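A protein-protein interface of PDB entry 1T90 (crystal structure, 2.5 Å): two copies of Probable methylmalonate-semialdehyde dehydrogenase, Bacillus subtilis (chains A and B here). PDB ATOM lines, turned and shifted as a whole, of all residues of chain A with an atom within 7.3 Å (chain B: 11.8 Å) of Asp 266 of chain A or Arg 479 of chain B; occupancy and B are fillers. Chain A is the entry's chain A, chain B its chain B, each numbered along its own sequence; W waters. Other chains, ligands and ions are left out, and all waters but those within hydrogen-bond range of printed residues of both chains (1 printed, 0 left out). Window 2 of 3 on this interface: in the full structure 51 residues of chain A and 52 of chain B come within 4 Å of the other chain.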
ATOM      1  N   ALA A 262       7.498 -10.185 -11.382  1.00  0.00           N
ATOM      2  CA  ALA A 262       7.160 -10.272  -9.970  1.00  0.00           C
ATOM      3  C   ALA A 262       7.474  -8.971  -9.245  1.00  0.00           C
ATOM      4  O   ALA A 262       8.359  -8.222  -9.658  1.00  0.00           O
ATOM      5  CB  ALA A 262       7.924 -11.414  -9.327  1.00  0.00           C
ATOM      6  N   ASN A 263       6.740  -8.703  -8.171  1.00  0.00           N
ATOM      7  CA  ASN A 263       6.957  -7.509  -7.364  1.00  0.00           C
ATOM      8  C   ASN A 263       8.024  -7.871  -6.333  1.00  0.00           C
ATOM      9  O   ASN A 263       7.710  -8.361  -5.248  1.00  0.00           O
ATOM     10  CB  ASN A 263       5.663  -7.101  -6.654  1.00  0.00           C
ATOM     11  CG  ASN A 263       5.861  -5.925  -5.708  1.00  0.00           C
ATOM     12  OD1 ASN A 263       6.696  -5.974  -4.800  1.00  0.00           O
ATOM     13  ND2 ASN A 263       5.092  -4.863  -5.912  1.00  0.00           N
ATOM     14  N   LEU A 264       9.281  -7.628  -6.686  1.00  0.00           N
ATOM     15  CA  LEU A 264      10.424  -7.945  -5.835  1.00  0.00           C
ATOM     16  C   LEU A 264      10.198  -7.758  -4.338  1.00  0.00           C
ATOM     17  O   LEU A 264      10.420  -8.681  -3.555  1.00  0.00           O
ATOM     18  CB  LEU A 264      11.636  -7.119  -6.279  1.00  0.00           C
ATOM     19  CG  LEU A 264      12.988  -7.833  -6.397  1.00  0.00           C
ATOM     20  CD1 LEU A 264      13.416  -8.359  -5.041  1.00  0.00           C
ATOM     21  CD2 LEU A 264      12.886  -8.970  -7.400  1.00  0.00           C
ATOM     22  N   GLU A 265       9.757  -6.569  -3.938  1.00  0.00           N
ATOM     23  CA  GLU A 265       9.527  -6.273  -2.523  1.00  0.00           C
ATOM     24  C   GLU A 265       8.608  -7.272  -1.829  1.00  0.00           C
ATOM     25  O   GLU A 265       8.986  -7.878  -0.824  1.00  0.00           O
ATOM     26  CB  GLU A 265       8.959  -4.861  -2.365  1.00  0.00           C
ATOM     27  CG  GLU A 265       9.861  -3.924  -1.571  1.00  0.00           C
ATOM     28  CD  GLU A 265      10.069  -4.384  -0.136  1.00  0.00           C
ATOM     29  OE1 GLU A 265       9.063  -4.532   0.591  1.00  0.00           O
ATOM     30  OE2 GLU A 265      11.234  -4.593   0.267  1.00  0.00           O
ATOM     31  N   ASP A 266       7.400  -7.436  -2.353  1.00  0.00           N
ATOM     32  CA  ASP A 266       6.459  -8.375  -1.763  1.00  0.00           C
ATOM     33  C   ASP A 266       7.014  -9.800  -1.827  1.00  0.00           C
ATOM     34  O   ASP A 266       7.005 -10.529  -0.832  1.00  0.00           O
ATOM     35  CB  ASP A 266       5.101  -8.318  -2.485  1.00  0.00           C
ATOM     36  CG  ASP A 266       4.310  -7.052  -2.164  1.00  0.00           C
ATOM     37  OD1 ASP A 266       4.315  -6.627  -0.987  1.00  0.00           O
ATOM     38  OD2 ASP A 266       3.666  -6.491  -3.083  1.00  0.00           O
ATOM     39  N   THR A 267       7.513 -10.184  -2.995  1.00  0.00           N
ATOM     40  CA  THR A 267       8.041 -11.526  -3.192  1.00  0.00           C
ATOM     41  C   THR A 267       9.083 -11.942  -2.155  1.00  0.00           C
ATOM     42  O   THR A 267       8.938 -12.974  -1.501  1.00  0.00           O
ATOM     43  CB  THR A 267       8.671 -11.670  -4.586  1.00  0.00           C
ATOM     44  OG1 THR A 267       7.792 -11.111  -5.568  1.00  0.00           O
ATOM     45  CG2 THR A 267       8.902 -13.139  -4.907  1.00  0.00           C
ATOM     46  N   VAL A 268      10.132 -11.140  -2.009  1.00  0.00           N
ATOM     47  CA  VAL A 268      11.195 -11.454  -1.066  1.00  0.00           C
ATOM     48  C   VAL A 268      10.723 -11.583   0.379  1.00  0.00           C
ATOM     49  O   VAL A 268      11.106 -12.521   1.075  1.00  0.00           O
ATOM     50  CB  VAL A 268      12.319 -10.413  -1.155  1.00  0.00           C
ATOM     51  CG1 VAL A 268      13.375 -10.682  -0.089  1.00  0.00           C
ATOM     52  CG2 VAL A 268      12.942 -10.471  -2.536  1.00  0.00           C
ATOM     53  N   THR A 269       9.896 -10.651   0.840  1.00  0.00           N
ATOM     54  CA  THR A 269       9.402 -10.732   2.211  1.00  0.00           C
ATOM     55  C   THR A 269       8.656 -12.048   2.397  1.00  0.00           C
ATOM     56  O   THR A 269       8.854 -12.760   3.391  1.00  0.00           O
ATOM     57  CB  THR A 269       8.445  -9.579   2.535  1.00  0.00           C
ATOM     58  OG1 THR A 269       9.154  -8.337   2.439  1.00  0.00           O
ATOM     59  CG2 THR A 269       7.890  -9.720   3.953  1.00  0.00           C
ATOM     60  N   ASN A 270       7.812 -12.370   1.420  1.00  0.00           N
ATOM     61  CA  ASN A 270       7.019 -13.593   1.443  1.00  0.00           C
ATOM     62  C   ASN A 270       7.863 -14.861   1.461  1.00  0.00           C
ATOM     63  O   ASN A 270       7.663 -15.735   2.311  1.00  0.00           O
ATOM     64  CB  ASN A 270       6.066 -13.614   0.243  1.00  0.00           C
ATOM     65  CG  ASN A 270       4.803 -12.807   0.492  1.00  0.00           C
ATOM     66  OD1 ASN A 270       3.885 -13.267   1.174  1.00  0.00           O
ATOM     67  ND2 ASN A 270       4.753 -11.598  -0.050  1.00  0.00           N
ATOM     68  N   ILE A 271       8.803 -14.962   0.527  1.00  0.00           N
ATOM     69  CA  ILE A 271       9.663 -16.133   0.449  1.00  0.00           C
ATOM     70  C   ILE A 271      10.516 -16.273   1.708  1.00  0.00           C
ATOM     71  O   ILE A 271      10.711 -17.384   2.208  1.00  0.00           O
ATOM     72  CB  ILE A 271      10.568 -16.074  -0.796  1.00  0.00           C
ATOM     73  CG1 ILE A 271       9.697 -16.042  -2.059  1.00  0.00           C
ATOM     74  CG2 ILE A 271      11.494 -17.286  -0.827  1.00  0.00           C
ATOM     75  CD1 ILE A 271      10.479 -15.924  -3.363  1.00  0.00           C
ATOM     76  N   VAL A 272      11.019 -15.154   2.230  1.00  0.00           N
ATOM     77  CA  VAL A 272      11.828 -15.201   3.447  1.00  0.00           C
ATOM     78  C   VAL A 272      10.985 -15.800   4.572  1.00  0.00           C
ATOM     79  O   VAL A 272      11.470 -16.618   5.353  1.00  0.00           O
ATOM     80  CB  VAL A 272      12.320 -13.794   3.871  1.00  0.00           C
ATOM     81  CG1 VAL A 272      13.012 -13.865   5.231  1.00  0.00           C
ATOM     82  CG2 VAL A 272      13.288 -13.252   2.835  1.00  0.00           C
ATOM     83  N   LYS A 302      18.256  -8.617  -3.026  1.00  0.00           N
ATOM     84  CA  LYS A 302      17.275  -8.266  -1.998  1.00  0.00           C
ATOM     85  C   LYS A 302      17.033  -9.386  -1.004  1.00  0.00           C
ATOM     86  O   LYS A 302      16.778  -9.127   0.171  1.00  0.00           O
ATOM     87  CB  LYS A 302      15.938  -7.859  -2.623  1.00  0.00           C
ATOM     88  CG  LYS A 302      15.950  -6.469  -3.222  1.00  0.00           C
ATOM     89  CD  LYS A 302      14.595  -5.792  -3.070  1.00  0.00           C
ATOM     90  CE  LYS A 302      14.225  -5.602  -1.604  1.00  0.00           C
ATOM     91  NZ  LYS A 302      12.966  -4.823  -1.467  1.00  0.00           N
ATOM     92  N   PHE A 414       5.005 -16.187  -8.246  1.00  0.00           N
ATOM     93  CA  PHE A 414       4.967 -14.748  -8.065  1.00  0.00           C
ATOM     94  C   PHE A 414       5.018 -14.139  -9.453  1.00  0.00           C
ATOM     95  O   PHE A 414       6.043 -14.198 -10.136  1.00  0.00           O
ATOM     96  CB  PHE A 414       6.141 -14.301  -7.201  1.00  0.00           C
ATOM     97  CG  PHE A 414       5.978 -14.661  -5.752  1.00  0.00           C
ATOM     98  CD1 PHE A 414       5.368 -13.777  -4.868  1.00  0.00           C
ATOM     99  CD2 PHE A 414       6.366 -15.915  -5.286  1.00  0.00           C
ATOM    100  CE1 PHE A 414       5.143 -14.137  -3.539  1.00  0.00           C
ATOM    101  CE2 PHE A 414       6.144 -16.284  -3.962  1.00  0.00           C
ATOM    102  CZ  PHE A 414       5.531 -15.395  -3.087  1.00  0.00           C
ATOM    103  N   THR A 415       3.878 -13.592  -9.870  1.00  0.00           N
ATOM    104  CA  THR A 415       3.726 -12.979 -11.183  1.00  0.00           C
ATOM    105  C   THR A 415       2.403 -12.233 -11.228  1.00  0.00           C
ATOM    106  O   THR A 415       1.592 -12.331 -10.307  1.00  0.00           O
ATOM    107  CB  THR A 415       3.703 -14.052 -12.293  1.00  0.00           C
ATOM    108  OG1 THR A 415       3.486 -13.434 -13.569  1.00  0.00           O
ATOM    109  CG2 THR A 415       2.589 -15.042 -12.037  1.00  0.00           C
ATOM    110  N   SER A 416       2.197 -11.480 -12.303  1.00  0.00           N
ATOM    111  CA  SER A 416       0.960 -10.742 -12.498  1.00  0.00           C
ATOM    112  C   SER A 416       0.443 -11.055 -13.891  1.00  0.00           C
ATOM    113  O   SER A 416      -0.445 -10.379 -14.408  1.00  0.00           O
ATOM    114  CB  SER A 416       1.189  -9.237 -12.347  1.00  0.00           C
ATOM    115  OG  SER A 416       1.321  -8.872 -10.981  1.00  0.00           O
ATOM    116  N   GLY A 434      -0.337 -21.290  -4.550  1.00  0.00           N
ATOM    117  CA  GLY A 434      -0.397 -19.939  -4.018  1.00  0.00           C
ATOM    118  C   GLY A 434       0.178 -18.909  -4.976  1.00  0.00           C
ATOM    119  O   GLY A 434       1.322 -19.026  -5.418  1.00  0.00           O
ATOM    120  N   ILE A 435      -0.618 -17.900  -5.309  1.00  0.00           N
ATOM    121  CA  ILE A 435      -0.174 -16.854  -6.217  1.00  0.00           C
ATOM    122  C   ILE A 435       0.120 -15.582  -5.419  1.00  0.00           C
ATOM    123  O   ILE A 435      -0.772 -15.011  -4.802  1.00  0.00           O
ATOM    124  CB  ILE A 435      -1.250 -16.539  -7.276  1.00  0.00           C
ATOM    125  CG1 ILE A 435      -1.763 -17.833  -7.917  1.00  0.00           C
ATOM    126  CG2 ILE A 435      -0.670 -15.616  -8.342  1.00  0.00           C
ATOM    127  CD1 ILE A 435      -0.717 -18.629  -8.660  1.00  0.00           C
ATOM    128  N   ASN A 436       1.377 -15.155  -5.432  1.00  0.00           N
ATOM    129  CA  ASN A 436       1.816 -13.961  -4.719  1.00  0.00           C
ATOM    130  C   ASN A 436       1.622 -14.072  -3.208  1.00  0.00           C
ATOM    131  O   ASN A 436       1.255 -13.106  -2.529  1.00  0.00           O
ATOM    132  CB  ASN A 436       1.108 -12.717  -5.264  1.00  0.00           C
ATOM    133  CG  ASN A 436       1.383 -12.495  -6.744  1.00  0.00           C
ATOM    134  OD1 ASN A 436       2.466 -12.813  -7.241  1.00  0.00           O
ATOM    135  ND2 ASN A 436       0.406 -11.938  -7.454  1.00  0.00           N
ATOM    136  N   LEU A 437       1.885 -15.270  -2.698  1.00  0.00           N
ATOM    137  CA  LEU A 437       1.782 -15.575  -1.279  1.00  0.00           C
ATOM    138  C   LEU A 437       2.879 -16.592  -1.002  1.00  0.00           C
ATOM    139  O   LEU A 437       3.111 -17.485  -1.815  1.00  0.00           O
ATOM    140  CB  LEU A 437       0.416 -16.181  -0.957  1.00  0.00           C
ATOM    141  CG  LEU A 437      -0.808 -15.264  -1.035  1.00  0.00           C
ATOM    142  CD1 LEU A 437      -2.078 -16.092  -0.899  1.00  0.00           C
ATOM    143  CD2 LEU A 437      -0.733 -14.215   0.062  1.00  0.00           C
ATOM    144  N   GLY A 438       3.552 -16.461   0.135  1.00  0.00           N
ATOM    145  CA  GLY A 438       4.631 -17.380   0.456  1.00  0.00           C
ATOM    146  C   GLY A 438       4.161 -18.736   0.936  1.00  0.00           C
ATOM    147  O   GLY A 438       4.746 -19.764   0.599  1.00  0.00           O
ATOM    148  N   LEU B 126     -14.409 -18.390  -3.870  1.00  0.00           N
ATOM    149  CA  LEU B 126     -14.718 -17.281  -2.984  1.00  0.00           C
ATOM    150  C   LEU B 126     -13.982 -16.059  -3.505  1.00  0.00           C
ATOM    151  O   LEU B 126     -12.782 -16.121  -3.771  1.00  0.00           O
ATOM    152  CB  LEU B 126     -14.274 -17.616  -1.556  1.00  0.00           C
ATOM    153  CG  LEU B 126     -15.347 -17.775  -0.466  1.00  0.00           C
ATOM    154  CD1 LEU B 126     -16.710 -18.083  -1.060  1.00  0.00           C
ATOM    155  CD2 LEU B 126     -14.914 -18.880   0.479  1.00  0.00           C
ATOM    156  N   ALA B 127     -14.704 -14.954  -3.667  1.00  0.00           N
ATOM    157  CA  ALA B 127     -14.108 -13.723  -4.177  1.00  0.00           C
ATOM    158  C   ALA B 127     -13.114 -13.097  -3.200  1.00  0.00           C
ATOM    159  O   ALA B 127     -12.149 -12.459  -3.618  1.00  0.00           O
ATOM    160  CB  ALA B 127     -15.199 -12.713  -4.523  1.00  0.00           C
ATOM    161  N   SER B 128     -13.340 -13.284  -1.903  1.00  0.00           N
ATOM    162  CA  SER B 128     -12.447 -12.711  -0.901  1.00  0.00           C
ATOM    163  C   SER B 128     -12.420 -13.483   0.414  1.00  0.00           C
ATOM    164  O   SER B 128     -13.434 -13.549   1.116  1.00  0.00           O
ATOM    165  CB  SER B 128     -12.854 -11.262  -0.598  1.00  0.00           C
ATOM    166  OG  SER B 128     -13.021 -10.507  -1.785  1.00  0.00           O
ATOM    167  N   ILE B 129     -11.266 -14.064   0.747  1.00  0.00           N
ATOM    168  CA  ILE B 129     -11.119 -14.783   2.012  1.00  0.00           C
ATOM    169  C   ILE B 129     -10.293 -13.900   2.950  1.00  0.00           C
ATOM    170  O   ILE B 129     -10.205 -14.136   4.154  1.00  0.00           O
ATOM    171  CB  ILE B 129     -10.409 -16.141   1.832  1.00  0.00           C
ATOM    172  CG1 ILE B 129      -9.012 -15.936   1.240  1.00  0.00           C
ATOM    173  CG2 ILE B 129     -11.263 -17.055   0.966  1.00  0.00           C
ATOM    174  CD1 ILE B 129      -8.167 -17.190   1.222  1.00  0.00           C
ATOM    175  N   ALA B 130      -9.692 -12.874   2.363  1.00  0.00           N
ATOM    176  CA  ALA B 130      -8.872 -11.897   3.072  1.00  0.00           C
ATOM    177  C   ALA B 130      -8.841 -10.711   2.123  1.00  0.00           C
ATOM    178  O   ALA B 130      -9.109 -10.876   0.934  1.00  0.00           O
ATOM    179  CB  ALA B 130      -7.467 -12.434   3.286  1.00  0.00           C
ATOM    180  N   THR B 131      -8.524  -9.525   2.624  1.00  0.00           N
ATOM    181  CA  THR B 131      -8.495  -8.371   1.739  1.00  0.00           C
ATOM    182  C   THR B 131      -7.500  -8.605   0.596  1.00  0.00           C
ATOM    183  O   THR B 131      -6.339  -8.952   0.822  1.00  0.00           O
ATOM    184  CB  THR B 131      -8.179  -7.046   2.517  1.00  0.00           C
ATOM    185  OG1 THR B 131      -7.100  -6.353   1.880  1.00  0.00           O
ATOM    186  CG2 THR B 131      -7.842  -7.328   3.967  1.00  0.00           C
ATOM    187  N   ASP B 132      -8.001  -8.456  -0.633  1.00  0.00           N
ATOM    188  CA  ASP B 132      -7.224  -8.642  -1.859  1.00  0.00           C
ATOM    189  C   ASP B 132      -6.824 -10.080  -2.181  1.00  0.00           C
ATOM    190  O   ASP B 132      -6.080 -10.317  -3.132  1.00  0.00           O
ATOM    191  CB  ASP B 132      -5.975  -7.765  -1.825  1.00  0.00           C
ATOM    192  CG  ASP B 132      -6.263  -6.340  -2.238  1.00  0.00           C
ATOM    193  OD1 ASP B 132      -5.446  -5.447  -1.902  1.00  0.00           O
ATOM    194  OD2 ASP B 132      -7.304  -6.120  -2.907  1.00  0.00           O
ATOM    195  N   VAL B 133      -7.322 -11.034  -1.404  1.00  0.00           N
ATOM    196  CA  VAL B 133      -7.000 -12.438  -1.625  1.00  0.00           C
ATOM    197  C   VAL B 133      -8.255 -13.215  -1.979  1.00  0.00           C
ATOM    198  O   VAL B 133      -9.281 -13.063  -1.331  1.00  0.00           O
ATOM    199  CB  VAL B 133      -6.374 -13.077  -0.359  1.00  0.00           C
ATOM    200  CG1 VAL B 133      -5.934 -14.501  -0.652  1.00  0.00           C
ATOM    201  CG2 VAL B 133      -5.204 -12.242   0.119  1.00  0.00           C
ATOM    202  N   GLU B 134      -8.167 -14.048  -3.009  1.00  0.00           N
ATOM    203  CA  GLU B 134      -9.298 -14.862  -3.438  1.00  0.00           C
ATOM    204  C   GLU B 134      -8.858 -16.325  -3.475  1.00  0.00           C
ATOM    205  O   GLU B 134      -7.667 -16.615  -3.636  1.00  0.00           O
ATOM    206  CB  GLU B 134      -9.779 -14.412  -4.816  1.00  0.00           C
ATOM    207  CG  GLU B 134      -8.837 -14.732  -5.964  1.00  0.00           C
ATOM    208  CD  GLU B 134      -9.110 -13.856  -7.175  1.00  0.00           C
ATOM    209  OE1 GLU B 134      -8.997 -14.351  -8.312  1.00  0.00           O
ATOM    210  OE2 GLU B 134      -9.431 -12.661  -6.985  1.00  0.00           O
ATOM    211  N   ALA B 135      -9.812 -17.242  -3.318  1.00  0.00           N
ATOM    212  CA  ALA B 135      -9.498 -18.666  -3.307  1.00  0.00           C
ATOM    213  C   ALA B 135     -10.577 -19.536  -3.924  1.00  0.00           C
ATOM    214  O   ALA B 135     -11.777 -19.308  -3.721  1.00  0.00           O
ATOM    215  CB  ALA B 135      -9.227 -19.128  -1.880  1.00  0.00           C
ATOM    216  N   ALA B 136     -10.137 -20.540  -4.672  1.00  0.00           N
ATOM    217  CA  ALA B 136     -11.041 -21.476  -5.322  1.00  0.00           C
ATOM    218  C   ALA B 136     -10.324 -22.798  -5.585  1.00  0.00           C
ATOM    219  O   ALA B 136      -9.105 -22.827  -5.768  1.00  0.00           O
ATOM    220  CB  ALA B 136     -11.545 -20.881  -6.638  1.00  0.00           C
ATOM    221  N   VAL B 475      -6.181 -26.465  -4.973  1.00  0.00           N
ATOM    222  CA  VAL B 475      -6.784 -25.259  -4.427  1.00  0.00           C
ATOM    223  C   VAL B 475      -5.823 -24.118  -4.747  1.00  0.00           C
ATOM    224  O   VAL B 475      -4.610 -24.262  -4.601  1.00  0.00           O
ATOM    225  CB  VAL B 475      -7.004 -25.379  -2.889  1.00  0.00           C
ATOM    226  CG1 VAL B 475      -5.719 -25.802  -2.203  1.00  0.00           C
ATOM    227  CG2 VAL B 475      -7.503 -24.058  -2.325  1.00  0.00           C
ATOM    228  N   VAL B 476      -6.364 -22.996  -5.207  1.00  0.00           N
ATOM    229  CA  VAL B 476      -5.541 -21.850  -5.557  1.00  0.00           C
ATOM    230  C   VAL B 476      -5.946 -20.629  -4.753  1.00  0.00           C
ATOM    231  O   VAL B 476      -7.066 -20.142  -4.877  1.00  0.00           O
ATOM    232  CB  VAL B 476      -5.663 -21.509  -7.069  1.00  0.00           C
ATOM    233  CG1 VAL B 476      -4.825 -20.289  -7.402  1.00  0.00           C
ATOM    234  CG2 VAL B 476      -5.211 -22.687  -7.906  1.00  0.00           C
ATOM    235  N   THR B 477      -5.033 -20.157  -3.913  1.00  0.00           N
ATOM    236  CA  THR B 477      -5.258 -18.970  -3.094  1.00  0.00           C
ATOM    237  C   THR B 477      -4.342 -17.916  -3.693  1.00  0.00           C
ATOM    238  O   THR B 477      -3.133 -18.107  -3.752  1.00  0.00           O
ATOM    239  CB  THR B 477      -4.862 -19.205  -1.626  1.00  0.00           C
ATOM    240  OG1 THR B 477      -5.583 -20.330  -1.115  1.00  0.00           O
ATOM    241  CG2 THR B 477      -5.198 -17.990  -0.782  1.00  0.00           C
ATOM    242  N   ALA B 478      -4.916 -16.811  -4.149  1.00  0.00           N
ATOM    243  CA  ALA B 478      -4.119 -15.772  -4.778  1.00  0.00           C
ATOM    244  C   ALA B 478      -4.338 -14.374  -4.214  1.00  0.00           C
ATOM    245  O   ALA B 478      -5.410 -14.050  -3.702  1.00  0.00           O
ATOM    246  CB  ALA B 478      -4.390 -15.766  -6.271  1.00  0.00           C
ATOM    247  N   ARG B 479      -3.303 -13.550  -4.321  1.00  0.00           N
ATOM    248  CA  ARG B 479      -3.357 -12.178  -3.853  1.00  0.00           C
ATOM    249  C   ARG B 479      -3.055 -11.250  -5.025  1.00  0.00           C
ATOM    250  O   ARG B 479      -1.949 -11.243  -5.568  1.00  0.00           O
ATOM    251  CB  ARG B 479      -2.350 -11.961  -2.724  1.00  0.00           C
ATOM    252  CG  ARG B 479      -2.160 -10.512  -2.335  1.00  0.00           C
ATOM    253  CD  ARG B 479      -1.438 -10.377  -1.007  1.00  0.00           C
ATOM    254  NE  ARG B 479      -1.011  -8.998  -0.787  1.00  0.00           N
ATOM    255  CZ  ARG B 479       0.067  -8.443  -1.344  1.00  0.00           C
ATOM    256  NH1 ARG B 479       0.368  -7.174  -1.087  1.00  0.00           N
ATOM    257  NH2 ARG B 479       0.859  -9.158  -2.138  1.00  0.00           N
ATOM    258  N   TYR B 480      -4.061 -10.487  -5.426  1.00  0.00           N
ATOM    259  CA  TYR B 480      -3.925  -9.546  -6.522  1.00  0.00           C
ATOM    260  C   TYR B 480      -4.246  -8.161  -5.982  1.00  0.00           C
ATOM    261  O   TYR B 480      -5.404  -7.732  -5.982  1.00  0.00           O
ATOM    262  CB  TYR B 480      -4.889  -9.913  -7.645  1.00  0.00           C
ATOM    263  CG  TYR B 480      -4.660 -11.301  -8.198  1.00  0.00           C
ATOM    264  CD1 TYR B 480      -5.689 -12.244  -8.223  1.00  0.00           C
ATOM    265  CD2 TYR B 480      -3.417 -11.670  -8.698  1.00  0.00           C
ATOM    266  CE1 TYR B 480      -5.484 -13.520  -8.735  1.00  0.00           C
ATOM    267  CE2 TYR B 480      -3.199 -12.942  -9.211  1.00  0.00           C
ATOM    268  CZ  TYR B 480      -4.234 -13.862  -9.229  1.00  0.00           C
ATOM    269  OH  TYR B 480      -4.014 -15.119  -9.749  1.00  0.00           O
ATOM    270  N   PRO B 481      -3.216  -7.449  -5.498  1.00  0.00           N
ATOM    271  CA  PRO B 481      -3.344  -6.102  -4.937  1.00  0.00           C
ATOM    272  C   PRO B 481      -4.056  -5.151  -5.888  1.00  0.00           C
ATOM    273  O   PRO B 481      -3.808  -5.155  -7.095  1.00  0.00           O
ATOM    274  CB  PRO B 481      -1.892  -5.690  -4.695  1.00  0.00           C
ATOM    275  CG  PRO B 481      -1.206  -6.990  -4.430  1.00  0.00           C
ATOM    276  CD  PRO B 481      -1.809  -7.886  -5.488  1.00  0.00           C
ATOM    277  N   ALA B 482      -4.951  -4.342  -5.342  1.00  0.00           N
ATOM    278  CA  ALA B 482      -5.677  -3.384  -6.157  1.00  0.00           C
ATOM    279  C   ALA B 482      -4.673  -2.356  -6.674  1.00  0.00           C
ATOM    280  O   ALA B 482      -3.952  -1.733  -5.891  1.00  0.00           O
ATOM    281  CB  ALA B 482      -6.754  -2.704  -5.326  1.00  0.00           C
ATOM    282  N   PRO B 483      -4.592  -2.179  -8.004  1.00  0.00           N
ATOM    283  CA  PRO B 483      -3.639  -1.201  -8.526  1.00  0.00           C
ATOM    284  C   PRO B 483      -3.996   0.239  -8.134  1.00  0.00           C
ATOM    285  O   PRO B 483      -5.142   0.541  -7.791  1.00  0.00           O
ATOM    286  CB  PRO B 483      -3.707  -1.438 -10.035  1.00  0.00           C
ATOM    287  CG  PRO B 483      -5.110  -1.893 -10.245  1.00  0.00           C
ATOM    288  CD  PRO B 483      -5.316  -2.846  -9.101  1.00  0.00           C
ATOM    289  N   ASP B 484      -2.995   1.116  -8.161  1.00  0.00           N
ATOM    290  CA  ASP B 484      -3.198   2.528  -7.841  1.00  0.00           C
ATOM    291  C   ASP B 484      -3.367   3.212  -9.184  1.00  0.00           C
ATOM    292  O   ASP B 484      -2.802   2.763 -10.183  1.00  0.00           O
ATOM    293  CB  ASP B 484      -1.970   3.116  -7.136  1.00  0.00           C
ATOM    294  CG  ASP B 484      -1.487   2.256  -5.989  1.00  0.00           C
ATOM    295  OD1 ASP B 484      -2.289   1.988  -5.069  1.00  0.00           O
ATOM    296  OD2 ASP B 484      -0.302   1.849  -6.010  1.00  0.00           O
HETATM  297  O   HOH W   1       2.077  -8.543  -4.469  1.00  0.00           O
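The side-chain carboxylate (OD2) of Asp 266 of chain A is in salt-bridge range of the guanidinium group (NH1) of Arg 479 of chain B (3.9 Å). The backbone NH (N) of Ile 435 of chain A lies within hydrogen-bond range of the backbone carbonyl oxygen (O) of Thr 477 of chain B, 3.0 Å away. N of Arg 479 of chain B is in hydrogen-bond range of O of Ile 435 of chain A (3.0 Å). O of Arg 479 of chain B is in hydrogen-bond range of ND2 of Asn 436 of chain A (3.1 Å).
The side-chain amide oxygen of Asn 263 of chain A sits at hydrogen-bond distance from the backbone NH of Asp 266 of chain A (2.9 Å). O of Asp 266 of chain A is in hydrogen-bond range of ND2 of Asn 270 of chain A, at 2.6 Å. The backbone NH (N) of Thr 415 of chain A sits at hydrogen-bond distance from the side-chain amide oxygen (OD1) of Asn 436 of chain A, 3.1 Å away. The backbone carbonyl oxygen of Asp 132 of chain B sits at hydrogen-bond distance from the backbone NH of Tyr 480 of chain B, at 3.1 Å. O of Glu 134 of chain B sits at hydrogen-bond distance from N of Ala 478 of chain B, at 2.8 Å. O of Ala 136 of chain B is in hydrogen-bond range of N of Val 476 of chain B, 2.8 Å away.
Among the printed residues, merely in contact across the chains: Gly 434 of chain A with Thr 477 of chain B (3.3 Å), Ile 435 of chain A with Val 476 of chain B (3.96 Å), Ile 435 of chain A with Ala 478 of chain B (3.4 Å), Ile 435 of chain A with Tyr 480 of chain B (3.7 Å), Leu 437 of chain A with Thr 477 of chain B (3.6 Å) and Leu 437 of chain A with Arg 479 of chain B (3.9 Å).
Asn 263 of chain A touches none of the printed residues of chain B. No residue of chain B comes within 4 Å of Leu 264 of chain A. Of chain B, only Arg 479 (3.9 Å) comes within 4 Å of Asp 266 of chain A. No residue of chain B comes within 4 Å of Thr 267 of chain A. No residue of chain B comes within 4 Å of Val 268 of chain A. No residue of chain B comes within 4 Å of Thr 269 of chain A. No residue of chain B comes within 4 Å of Asn 270 of chain A. Ile 271 of chain A touches none of the printed residues of chain B. Of the printed residues of chain B, Gly 434 of chain A touches Thr 477 (3.3 Å). Printed residues of chain B within 4 Å of Ile 435 of chain A: Val 476, Thr 477, Ala 478, Arg 479 and Tyr 480. Asn 436 of chain A touches just one residue of chain B: Arg 479. Printed residues of chain A within 4 Å of Thr 477 of chain B: Gly 434, Ile 435 and Leu 437. Of chain A, only Asp 266, Ile 435, Asn 436 and Leu 437 come within 4 Å of Arg 479 of chain B. Printed residues of chain A within 4 Å of Tyr 480 of chain B: Ile 435 (3.7 Å). Pro 483 of chain B touches none of the printed residues of chain A. The nearest residue of chain A that does not touch Arg 479 of chain B is Asn 270 of chain A (5.0 Å). The nearest printed residue of chain B that does not touch Gly 434 of chain A is Val 475 of chain B (5.2 Å).
Printed residues of chain B that touch a printed residue of chain A: Val 476, Thr 477, Ala 478, Arg 479 and Tyr 480. Of the 20 printed residues of chain A, 5 touch a printed residue of chain B. Printed residues of chain A that touch a printed residue of chain B: Asp 266, Gly 434, Ile 435, Asn 436 and Leu 437. Hydrophobic or aromatic side chains of chain A within 4 Å of the printed part of chain B: Ile 435 and Leu 437. Among the printed residues, Asp or Glu carboxylates within 4 Å of a Lys or Arg side-chain nitrogen of the other chain: Asp 266 of chain A with Arg 479 of chain B (3.9 Å).
No position is printed for both chains.
Water W1 lies within hydrogen-bond range of NH2 of Arg 479 of chain B and OD2 of Asp 266 of chain A.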
